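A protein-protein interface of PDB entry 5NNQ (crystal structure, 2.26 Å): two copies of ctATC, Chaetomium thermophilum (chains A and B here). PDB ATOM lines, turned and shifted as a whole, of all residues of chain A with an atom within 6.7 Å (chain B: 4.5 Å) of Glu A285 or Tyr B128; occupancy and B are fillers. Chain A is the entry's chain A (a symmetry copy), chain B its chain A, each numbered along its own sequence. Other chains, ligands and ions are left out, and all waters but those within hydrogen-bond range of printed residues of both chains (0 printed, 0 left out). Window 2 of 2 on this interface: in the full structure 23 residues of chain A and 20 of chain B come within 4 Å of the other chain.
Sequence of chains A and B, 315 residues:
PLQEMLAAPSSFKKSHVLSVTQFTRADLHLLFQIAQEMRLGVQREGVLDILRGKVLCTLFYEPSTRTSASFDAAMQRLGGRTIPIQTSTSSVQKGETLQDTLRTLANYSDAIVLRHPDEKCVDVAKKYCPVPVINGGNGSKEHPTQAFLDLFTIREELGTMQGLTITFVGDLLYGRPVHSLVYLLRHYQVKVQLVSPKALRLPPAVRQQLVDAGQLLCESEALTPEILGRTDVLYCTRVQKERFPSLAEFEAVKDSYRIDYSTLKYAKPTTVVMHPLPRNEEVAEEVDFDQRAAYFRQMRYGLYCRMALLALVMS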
ATOM      1  N   ARG A 258      -5.033  -4.788 -39.872  1.00  0.00           N
ATOM      2  CA  ARG A 258      -4.793  -5.099 -38.472  1.00  0.00           C
ATOM      3  C   ARG A 258      -3.461  -4.507 -38.024  1.00  0.00           C
ATOM      4  O   ARG A 258      -2.425  -4.760 -38.638  1.00  0.00           O
ATOM      5  CB  ARG A 258      -4.812  -6.615 -38.288  1.00  0.00           C
ATOM      6  CG  ARG A 258      -4.726  -7.079 -36.857  1.00  0.00           C
ATOM      7  CD  ARG A 258      -5.184  -8.531 -36.702  1.00  0.00           C
ATOM      8  NE  ARG A 258      -4.483  -9.247 -35.615  1.00  0.00           N
ATOM      9  CZ  ARG A 258      -4.878  -9.318 -34.333  1.00  0.00           C
ATOM     10  NH1 ARG A 258      -5.985  -8.710 -33.906  1.00  0.00           N
ATOM     11  NH2 ARG A 258      -4.149 -10.009 -33.456  1.00  0.00           N
ATOM     12  N   ILE A 259      -3.516  -3.656 -37.000  1.00  0.00           N
ATOM     13  CA  ILE A 259      -2.340  -3.116 -36.319  1.00  0.00           C
ATOM     14  C   ILE A 259      -1.866  -4.175 -35.337  1.00  0.00           C
ATOM     15  O   ILE A 259      -2.502  -4.385 -34.292  1.00  0.00           O
ATOM     16  CB  ILE A 259      -2.653  -1.807 -35.600  1.00  0.00           C
ATOM     17  CG1 ILE A 259      -3.378  -0.855 -36.544  1.00  0.00           C
ATOM     18  CG2 ILE A 259      -1.371  -1.205 -35.095  1.00  0.00           C
ATOM     19  CD1 ILE A 259      -2.770  -0.864 -37.965  1.00  0.00           C
ATOM     20  N   TYR A 261       2.318  -6.356 -34.363  1.00  0.00           N
ATOM     21  CA  TYR A 261       3.750  -6.032 -34.308  1.00  0.00           C
ATOM     22  C   TYR A 261       4.353  -5.979 -35.704  1.00  0.00           C
ATOM     23  O   TYR A 261       5.089  -5.033 -36.038  1.00  0.00           O
ATOM     24  CB  TYR A 261       4.503  -7.030 -33.392  1.00  0.00           C
ATOM     25  CG  TYR A 261       4.463  -6.587 -31.929  1.00  0.00           C
ATOM     26  CD1 TYR A 261       4.779  -5.259 -31.564  1.00  0.00           C
ATOM     27  CD2 TYR A 261       4.075  -7.468 -30.915  1.00  0.00           C
ATOM     28  CE1 TYR A 261       4.724  -4.834 -30.220  1.00  0.00           C
ATOM     29  CE2 TYR A 261       4.018  -7.054 -29.572  1.00  0.00           C
ATOM     30  CZ  TYR A 261       4.336  -5.745 -29.234  1.00  0.00           C
ATOM     31  OH  TYR A 261       4.284  -5.369 -27.906  1.00  0.00           O
ATOM     32  N   ARG A 279     -13.206  -1.608 -30.079  1.00  0.00           N
ATOM     33  CA  ARG A 279     -12.484  -2.230 -31.180  1.00  0.00           C
ATOM     34  C   ARG A 279     -12.903  -3.690 -31.293  1.00  0.00           C
ATOM     35  O   ARG A 279     -13.302  -4.300 -30.296  1.00  0.00           O
ATOM     36  CB  ARG A 279     -10.958  -2.167 -30.945  1.00  0.00           C
ATOM     37  CG  ARG A 279     -10.519  -2.883 -29.626  1.00  0.00           C
ATOM     38  CD  ARG A 279      -9.025  -3.344 -29.581  1.00  0.00           C
ATOM     39  NE  ARG A 279      -8.621  -3.476 -28.178  1.00  0.00           N
ATOM     40  CZ  ARG A 279      -7.400  -3.695 -27.728  1.00  0.00           C
ATOM     41  NH1 ARG A 279      -6.371  -3.843 -28.559  1.00  0.00           N
ATOM     42  NH2 ARG A 279      -7.226  -3.762 -26.431  1.00  0.00           N
ATOM     43  N   GLU A 281     -10.891  -6.673 -33.779  1.00  0.00           N
ATOM     44  CA  GLU A 281      -9.547  -7.221 -33.871  1.00  0.00           C
ATOM     45  C   GLU A 281      -8.611  -6.320 -34.666  1.00  0.00           C
ATOM     46  O   GLU A 281      -7.507  -6.743 -34.989  1.00  0.00           O
ATOM     47  CB  GLU A 281      -9.596  -8.611 -34.510  1.00  0.00           C
ATOM     48  CG  GLU A 281     -10.331  -9.647 -33.706  1.00  0.00           C
ATOM     49  CD  GLU A 281      -9.614  -9.960 -32.411  1.00  0.00           C
ATOM     50  OE1 GLU A 281      -8.378  -9.751 -32.349  1.00  0.00           O
ATOM     51  OE2 GLU A 281     -10.279 -10.402 -31.450  1.00  0.00           O
ATOM     52  N   VAL A 283      -7.021  -3.726 -33.838  1.00  0.00           N
ATOM     53  CA  VAL A 283      -5.786  -3.487 -33.089  1.00  0.00           C
ATOM     54  C   VAL A 283      -5.557  -4.672 -32.167  1.00  0.00           C
ATOM     55  O   VAL A 283      -6.371  -4.943 -31.273  1.00  0.00           O
ATOM     56  CB  VAL A 283      -5.807  -2.174 -32.320  1.00  0.00           C
ATOM     57  CG1 VAL A 283      -4.485  -2.017 -31.527  1.00  0.00           C
ATOM     58  CG2 VAL A 283      -5.942  -1.076 -33.314  1.00  0.00           C
ATOM     59  N   ALA A 284      -4.474  -5.402 -32.422  1.00  0.00           N
ATOM     60  CA  ALA A 284      -4.176  -6.610 -31.674  1.00  0.00           C
ATOM     61  C   ALA A 284      -3.845  -6.283 -30.213  1.00  0.00           C
ATOM     62  O   ALA A 284      -3.251  -5.232 -29.896  1.00  0.00           O
ATOM     63  CB  ALA A 284      -3.009  -7.356 -32.334  1.00  0.00           C
ATOM     64  N   GLU A 285      -4.260  -7.196 -29.324  1.00  0.00           N
ATOM     65  CA  GLU A 285      -3.952  -7.082 -27.892  1.00  0.00           C
ATOM     66  C   GLU A 285      -2.446  -7.045 -27.635  1.00  0.00           C
ATOM     67  O   GLU A 285      -1.973  -6.281 -26.768  1.00  0.00           O
ATOM     68  CB  GLU A 285      -4.586  -8.245 -27.120  1.00  0.00           C
ATOM     69  CG  GLU A 285      -6.113  -8.055 -26.971  1.00  0.00           C
ATOM     70  CD  GLU A 285      -6.743  -8.724 -25.725  1.00  0.00           C
ATOM     71  OE1 GLU A 285      -6.029  -9.142 -24.766  1.00  0.00           O
ATOM     72  OE2 GLU A 285      -7.997  -8.811 -25.718  1.00  0.00           O
ATOM     73  N   GLU A 286      -1.673  -7.800 -28.443  1.00  0.00           N
ATOM     74  CA  GLU A 286      -0.211  -7.848 -28.303  1.00  0.00           C
ATOM     75  C   GLU A 286       0.423  -6.467 -28.376  1.00  0.00           C
ATOM     76  O   GLU A 286       1.575  -6.306 -27.976  1.00  0.00           O
ATOM     77  CB  GLU A 286       0.387  -8.767 -29.365  1.00  0.00           C
ATOM     78  CG  GLU A 286       0.613  -8.123 -30.757  1.00  0.00           C
ATOM     79  CD  GLU A 286       1.200  -9.100 -31.754  1.00  0.00           C
ATOM     80  OE1 GLU A 286       1.519 -10.237 -31.341  1.00  0.00           O
ATOM     81  OE2 GLU A 286       1.348  -8.749 -32.947  1.00  0.00           O
ATOM     82  N   VAL A 287      -0.330  -5.458 -28.815  1.00  0.00           N
ATOM     83  CA  VAL A 287       0.184  -4.114 -28.965  1.00  0.00           C
ATOM     84  C   VAL A 287      -0.205  -3.201 -27.813  1.00  0.00           C
ATOM     85  O   VAL A 287       0.325  -2.079 -27.717  1.00  0.00           O
ATOM     86  CB  VAL A 287      -0.285  -3.604 -30.350  1.00  0.00           C
ATOM     87  CG1 VAL A 287      -0.454  -2.092 -30.444  1.00  0.00           C
ATOM     88  CG2 VAL A 287       0.689  -4.161 -31.419  1.00  0.00           C
ATOM     89  N   ASP A 288      -1.046  -3.661 -26.887  1.00  0.00           N
ATOM     90  CA  ASP A 288      -1.633  -2.735 -25.906  1.00  0.00           C
ATOM     91  C   ASP A 288      -0.599  -2.142 -24.959  1.00  0.00           C
ATOM     92  O   ASP A 288      -0.825  -1.066 -24.385  1.00  0.00           O
ATOM     93  CB  ASP A 288      -2.687  -3.456 -25.043  1.00  0.00           C
ATOM     94  CG  ASP A 288      -3.956  -3.881 -25.813  1.00  0.00           C
ATOM     95  OD1 ASP A 288      -4.142  -3.561 -27.001  1.00  0.00           O
ATOM     96  OD2 ASP A 288      -4.765  -4.593 -25.197  1.00  0.00           O
ATOM     97  N   PHE A 289       0.458  -2.876 -24.677  1.00  0.00           N
ATOM     98  CA  PHE A 289       1.458  -2.417 -23.725  1.00  0.00           C
ATOM     99  C   PHE A 289       2.534  -1.581 -24.393  1.00  0.00           C
ATOM    100  O   PHE A 289       3.384  -1.018 -23.695  1.00  0.00           O
ATOM    101  CB  PHE A 289       2.055  -3.633 -22.997  1.00  0.00           C
ATOM    102  CG  PHE A 289       1.213  -4.076 -21.828  1.00  0.00           C
ATOM    103  CD1 PHE A 289       0.994  -3.204 -20.772  1.00  0.00           C
ATOM    104  CD2 PHE A 289       0.596  -5.312 -21.803  1.00  0.00           C
ATOM    105  CE1 PHE A 289       0.188  -3.564 -19.691  1.00  0.00           C
ATOM    106  CE2 PHE A 289      -0.201  -5.672 -20.731  1.00  0.00           C
ATOM    107  CZ  PHE A 289      -0.389  -4.775 -19.671  1.00  0.00           C
ATOM    108  N   ASP A 290       2.478  -1.468 -25.728  1.00  0.00           N
ATOM    109  CA  ASP A 290       3.454  -0.700 -26.477  1.00  0.00           C
ATOM    110  C   ASP A 290       3.223   0.751 -26.183  1.00  0.00           C
ATOM    111  O   ASP A 290       2.078   1.206 -26.108  1.00  0.00           O
ATOM    112  CB  ASP A 290       3.346  -1.019 -27.965  1.00  0.00           C
ATOM    113  CG  ASP A 290       4.397  -0.323 -28.839  1.00  0.00           C
ATOM    114  OD1 ASP A 290       4.397   0.930 -28.968  1.00  0.00           O
ATOM    115  OD2 ASP A 290       5.183  -1.074 -29.446  1.00  0.00           O
ATOM    116  N   TYR A 295      -4.754   4.450 -27.091  1.00  0.00           N
ATOM    117  CA  TYR A 295      -6.219   4.398 -27.016  1.00  0.00           C
ATOM    118  C   TYR A 295      -6.785   4.255 -25.601  1.00  0.00           C
ATOM    119  O   TYR A 295      -7.983   4.494 -25.411  1.00  0.00           O
ATOM    120  CB  TYR A 295      -6.745   3.253 -27.867  1.00  0.00           C
ATOM    121  CG  TYR A 295      -5.878   2.014 -28.015  1.00  0.00           C
ATOM    122  CD1 TYR A 295      -4.944   1.930 -29.025  1.00  0.00           C
ATOM    123  CD2 TYR A 295      -6.045   0.905 -27.183  1.00  0.00           C
ATOM    124  CE1 TYR A 295      -4.169   0.792 -29.198  1.00  0.00           C
ATOM    125  CE2 TYR A 295      -5.286  -0.242 -27.355  1.00  0.00           C
ATOM    126  CZ  TYR A 295      -4.322  -0.282 -28.370  1.00  0.00           C
ATOM    127  OH  TYR A 295      -3.537  -1.430 -28.571  1.00  0.00           O
ATOM    128  N   GLN B  99     -11.044  -6.851 -20.235  1.00  0.00           N
ATOM    129  CA  GLN B  99      -9.795  -6.090 -20.063  1.00  0.00           C
ATOM    130  C   GLN B  99      -9.908  -4.696 -20.669  1.00  0.00           C
ATOM    131  O   GLN B  99      -9.393  -3.722 -20.094  1.00  0.00           O
ATOM    132  CB  GLN B  99      -8.600  -6.850 -20.650  1.00  0.00           C
ATOM    133  CG  GLN B  99      -8.794  -7.329 -22.096  1.00  0.00           C
ATOM    134  CD  GLN B  99      -9.243  -8.763 -22.151  1.00  0.00           C
ATOM    135  OE1 GLN B  99     -10.276  -9.176 -21.555  1.00  0.00           O
ATOM    136  NE2 GLN B  99      -8.479  -9.541 -22.868  1.00  0.00           N
ATOM    137  N   ARG B 103      -9.653  -1.308 -18.340  1.00  0.00           N
ATOM    138  CA  ARG B 103      -8.726  -0.221 -18.646  1.00  0.00           C
ATOM    139  C   ARG B 103      -9.475   1.063 -18.970  1.00  0.00           C
ATOM    140  O   ARG B 103      -9.043   2.142 -18.579  1.00  0.00           O
ATOM    141  CB  ARG B 103      -7.790  -0.683 -19.759  1.00  0.00           C
ATOM    142  CG  ARG B 103      -6.625  -1.671 -19.213  1.00  0.00           C
ATOM    143  CD  ARG B 103      -5.868  -2.332 -20.350  1.00  0.00           C
ATOM    144  NE  ARG B 103      -6.725  -3.155 -21.197  1.00  0.00           N
ATOM    145  CZ  ARG B 103      -6.298  -3.879 -22.217  1.00  0.00           C
ATOM    146  NH1 ARG B 103      -4.995  -3.921 -22.511  1.00  0.00           N
ATOM    147  NH2 ARG B 103      -7.164  -4.608 -22.929  1.00  0.00           N
ATOM    148  N   VAL B 124      -7.490 -11.725 -15.339  1.00  0.00           N
ATOM    149  CA  VAL B 124      -7.575 -10.612 -16.272  1.00  0.00           C
ATOM    150  C   VAL B 124      -7.322  -9.326 -15.527  1.00  0.00           C
ATOM    151  O   VAL B 124      -6.510  -8.499 -15.954  1.00  0.00           O
ATOM    152  CB  VAL B 124      -8.946 -10.632 -16.995  1.00  0.00           C
ATOM    153  CG1 VAL B 124      -9.125  -9.420 -17.881  1.00  0.00           C
ATOM    154  CG2 VAL B 124      -9.046 -11.869 -17.884  1.00  0.00           C
ATOM    155  N   ALA B 125      -7.933  -9.173 -14.338  1.00  0.00           N
ATOM    156  CA  ALA B 125      -7.812  -7.889 -13.649  1.00  0.00           C
ATOM    157  C   ALA B 125      -6.385  -7.659 -13.207  1.00  0.00           C
ATOM    158  O   ALA B 125      -5.931  -6.508 -13.108  1.00  0.00           O
ATOM    159  CB  ALA B 125      -8.725  -7.837 -12.412  1.00  0.00           C
ATOM    160  N   LYS B 126      -5.692  -8.748 -12.891  1.00  0.00           N
ATOM    161  CA  LYS B 126      -4.331  -8.627 -12.413  1.00  0.00           C
ATOM    162  C   LYS B 126      -3.412  -8.267 -13.572  1.00  0.00           C
ATOM    163  O   LYS B 126      -2.629  -7.328 -13.463  1.00  0.00           O
ATOM    164  CB  LYS B 126      -3.904  -9.933 -11.712  1.00  0.00           C
ATOM    165  CG  LYS B 126      -2.710  -9.749 -10.749  1.00  0.00           C
ATOM    166  CD  LYS B 126      -2.227 -11.068 -10.117  1.00  0.00           C
ATOM    167  CE  LYS B 126      -0.867 -10.874  -9.400  1.00  0.00           C
ATOM    168  NZ  LYS B 126      -0.876  -9.895  -8.242  1.00  0.00           N
ATOM    169  N   LYS B 127      -3.571  -8.942 -14.722  1.00  0.00           N
ATOM    170  CA  LYS B 127      -2.728  -8.638 -15.884  1.00  0.00           C
ATOM    171  C   LYS B 127      -2.930  -7.235 -16.466  1.00  0.00           C
ATOM    172  O   LYS B 127      -1.980  -6.684 -17.019  1.00  0.00           O
ATOM    173  CB  LYS B 127      -3.000  -9.648 -16.984  1.00  0.00           C
ATOM    174  CG  LYS B 127      -2.093  -9.490 -18.215  1.00  0.00           C
ATOM    175  CD  LYS B 127      -2.199 -10.749 -19.063  1.00  0.00           C
ATOM    176  CE  LYS B 127      -1.582 -10.596 -20.452  1.00  0.00           C
ATOM    177  NZ  LYS B 127      -2.323 -11.433 -21.463  1.00  0.00           N
ATOM    178  N   TYR B 128      -4.154  -6.631 -16.399  1.00  0.00           N
ATOM    179  CA  TYR B 128      -4.434  -5.478 -17.253  1.00  0.00           C
ATOM    180  C   TYR B 128      -4.809  -4.213 -16.516  1.00  0.00           C
ATOM    181  O   TYR B 128      -4.534  -3.125 -17.024  1.00  0.00           O
ATOM    182  CB  TYR B 128      -5.552  -5.806 -18.243  1.00  0.00           C
ATOM    183  CG  TYR B 128      -5.163  -6.717 -19.337  1.00  0.00           C
ATOM    184  CD1 TYR B 128      -4.325  -6.281 -20.336  1.00  0.00           C
ATOM    185  CD2 TYR B 128      -5.629  -8.034 -19.389  1.00  0.00           C
ATOM    186  CE1 TYR B 128      -3.964  -7.126 -21.373  1.00  0.00           C
ATOM    187  CE2 TYR B 128      -5.253  -8.881 -20.402  1.00  0.00           C
ATOM    188  CZ  TYR B 128      -4.415  -8.399 -21.409  1.00  0.00           C
ATOM    189  OH  TYR B 128      -4.021  -9.208 -22.450  1.00  0.00           O
ATOM    190  N   CYS B 129      -5.364  -4.312 -15.376  1.00  0.00           N
ATOM    191  CA  CYS B 129      -5.990  -3.178 -14.738  1.00  0.00           C
ATOM    192  C   CYS B 129      -4.963  -2.417 -13.895  1.00  0.00           C
ATOM    193  O   CYS B 129      -4.336  -3.013 -13.017  1.00  0.00           O
ATOM    194  CB  CYS B 129      -7.172  -3.617 -13.834  1.00  0.00           C
ATOM    195  SG  CYS B 129      -8.137  -2.198 -13.183  1.00  0.00           S
ATOM    196  N   PRO B 130      -4.823  -1.117 -14.106  1.00  0.00           N
ATOM    197  CA  PRO B 130      -3.795  -0.335 -13.403  1.00  0.00           C
ATOM    198  C   PRO B 130      -4.288   0.329 -12.138  1.00  0.00           C
ATOM    199  O   PRO B 130      -3.660   1.290 -11.719  1.00  0.00           O
ATOM    200  CB  PRO B 130      -3.418   0.742 -14.440  1.00  0.00           C
ATOM    201  CG  PRO B 130      -4.791   0.995 -15.181  1.00  0.00           C
ATOM    202  CD  PRO B 130      -5.456  -0.349 -15.214  1.00  0.00           C
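Of chain B, only Gln B99 (3.0 Å) and Tyr B128 (3.1 Å) come within 4 Å of Glu A285. Printed residues of chain B within 4 Å of Asp A288: Arg B103. Tyr A295 touches none of the printed residues of chain B. Of the printed residues of chain A, Gln B99 touches Glu A285. Of the printed residues of chain A, Arg B103 touches Arg A279 (3.6 Å) and Asp A288 (2.8 Å). Of the printed residues of chain A, Tyr B128 touches Glu A285. Cys B129 touches none of the printed residues of chain A. The nearest printed residue of chain B that does not touch Glu A285 is Arg B103 (5.0 Å). The nearest residue of chain A that does not touch Tyr B128 is Phe A289 (4.1 Å).
Hydrophobic or aromatic side chains of chain A that line the printed part of chain B: Phe A289. Of the 9 printed residues of chain B, 4 touch a printed residue of chain A. Hydrophobic or aromatic side chains of chain B that line the printed part of chain A: Tyr B128. Among the printed residues, 5 pairs touch across the chains.
The backbone carbonyl oxygen of Gln B99 sits at hydrogen-bond distance from the guanidinium group of Arg B103 (2.9 Å). The side-chain hydroxyl (OH) of Tyr B128 lies within hydrogen-bond range of the side-chain amino group (NZ) of Lys B127, at 3.0 Å. The guanidinium group of Arg A279 lies within hydrogen-bond range of the backbone carbonyl oxygen of Val A283, 2.9 Å away. The guanidinium group (NH1) of Arg A279 is in salt-bridge range of the side-chain carboxylate (OD1) of Asp A288, at 2.7 Å. OD1 of Asp A288 is in hydrogen-bond range of OH of Tyr A295 (2.7 Å).
Among the printed residues, merely in contact across the chains: Arg A279 with Arg B103 and Phe A289 with Lys B127.
The side-chain carboxylate (OE2) of Glu A285 lies within hydrogen-bond range of the side-chain amide nitrogen (NE2) of Gln B99 (3.0 Å). The side-chain carboxylate (OD2) of Asp A288 lies within salt-bridge range of the guanidinium group (NH1) of Arg B103 (2.8 Å). OH of Tyr B128 sits at hydrogen-bond distance from OE1 of Glu A285 (3.1 Å).
No position is printed for both chains.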
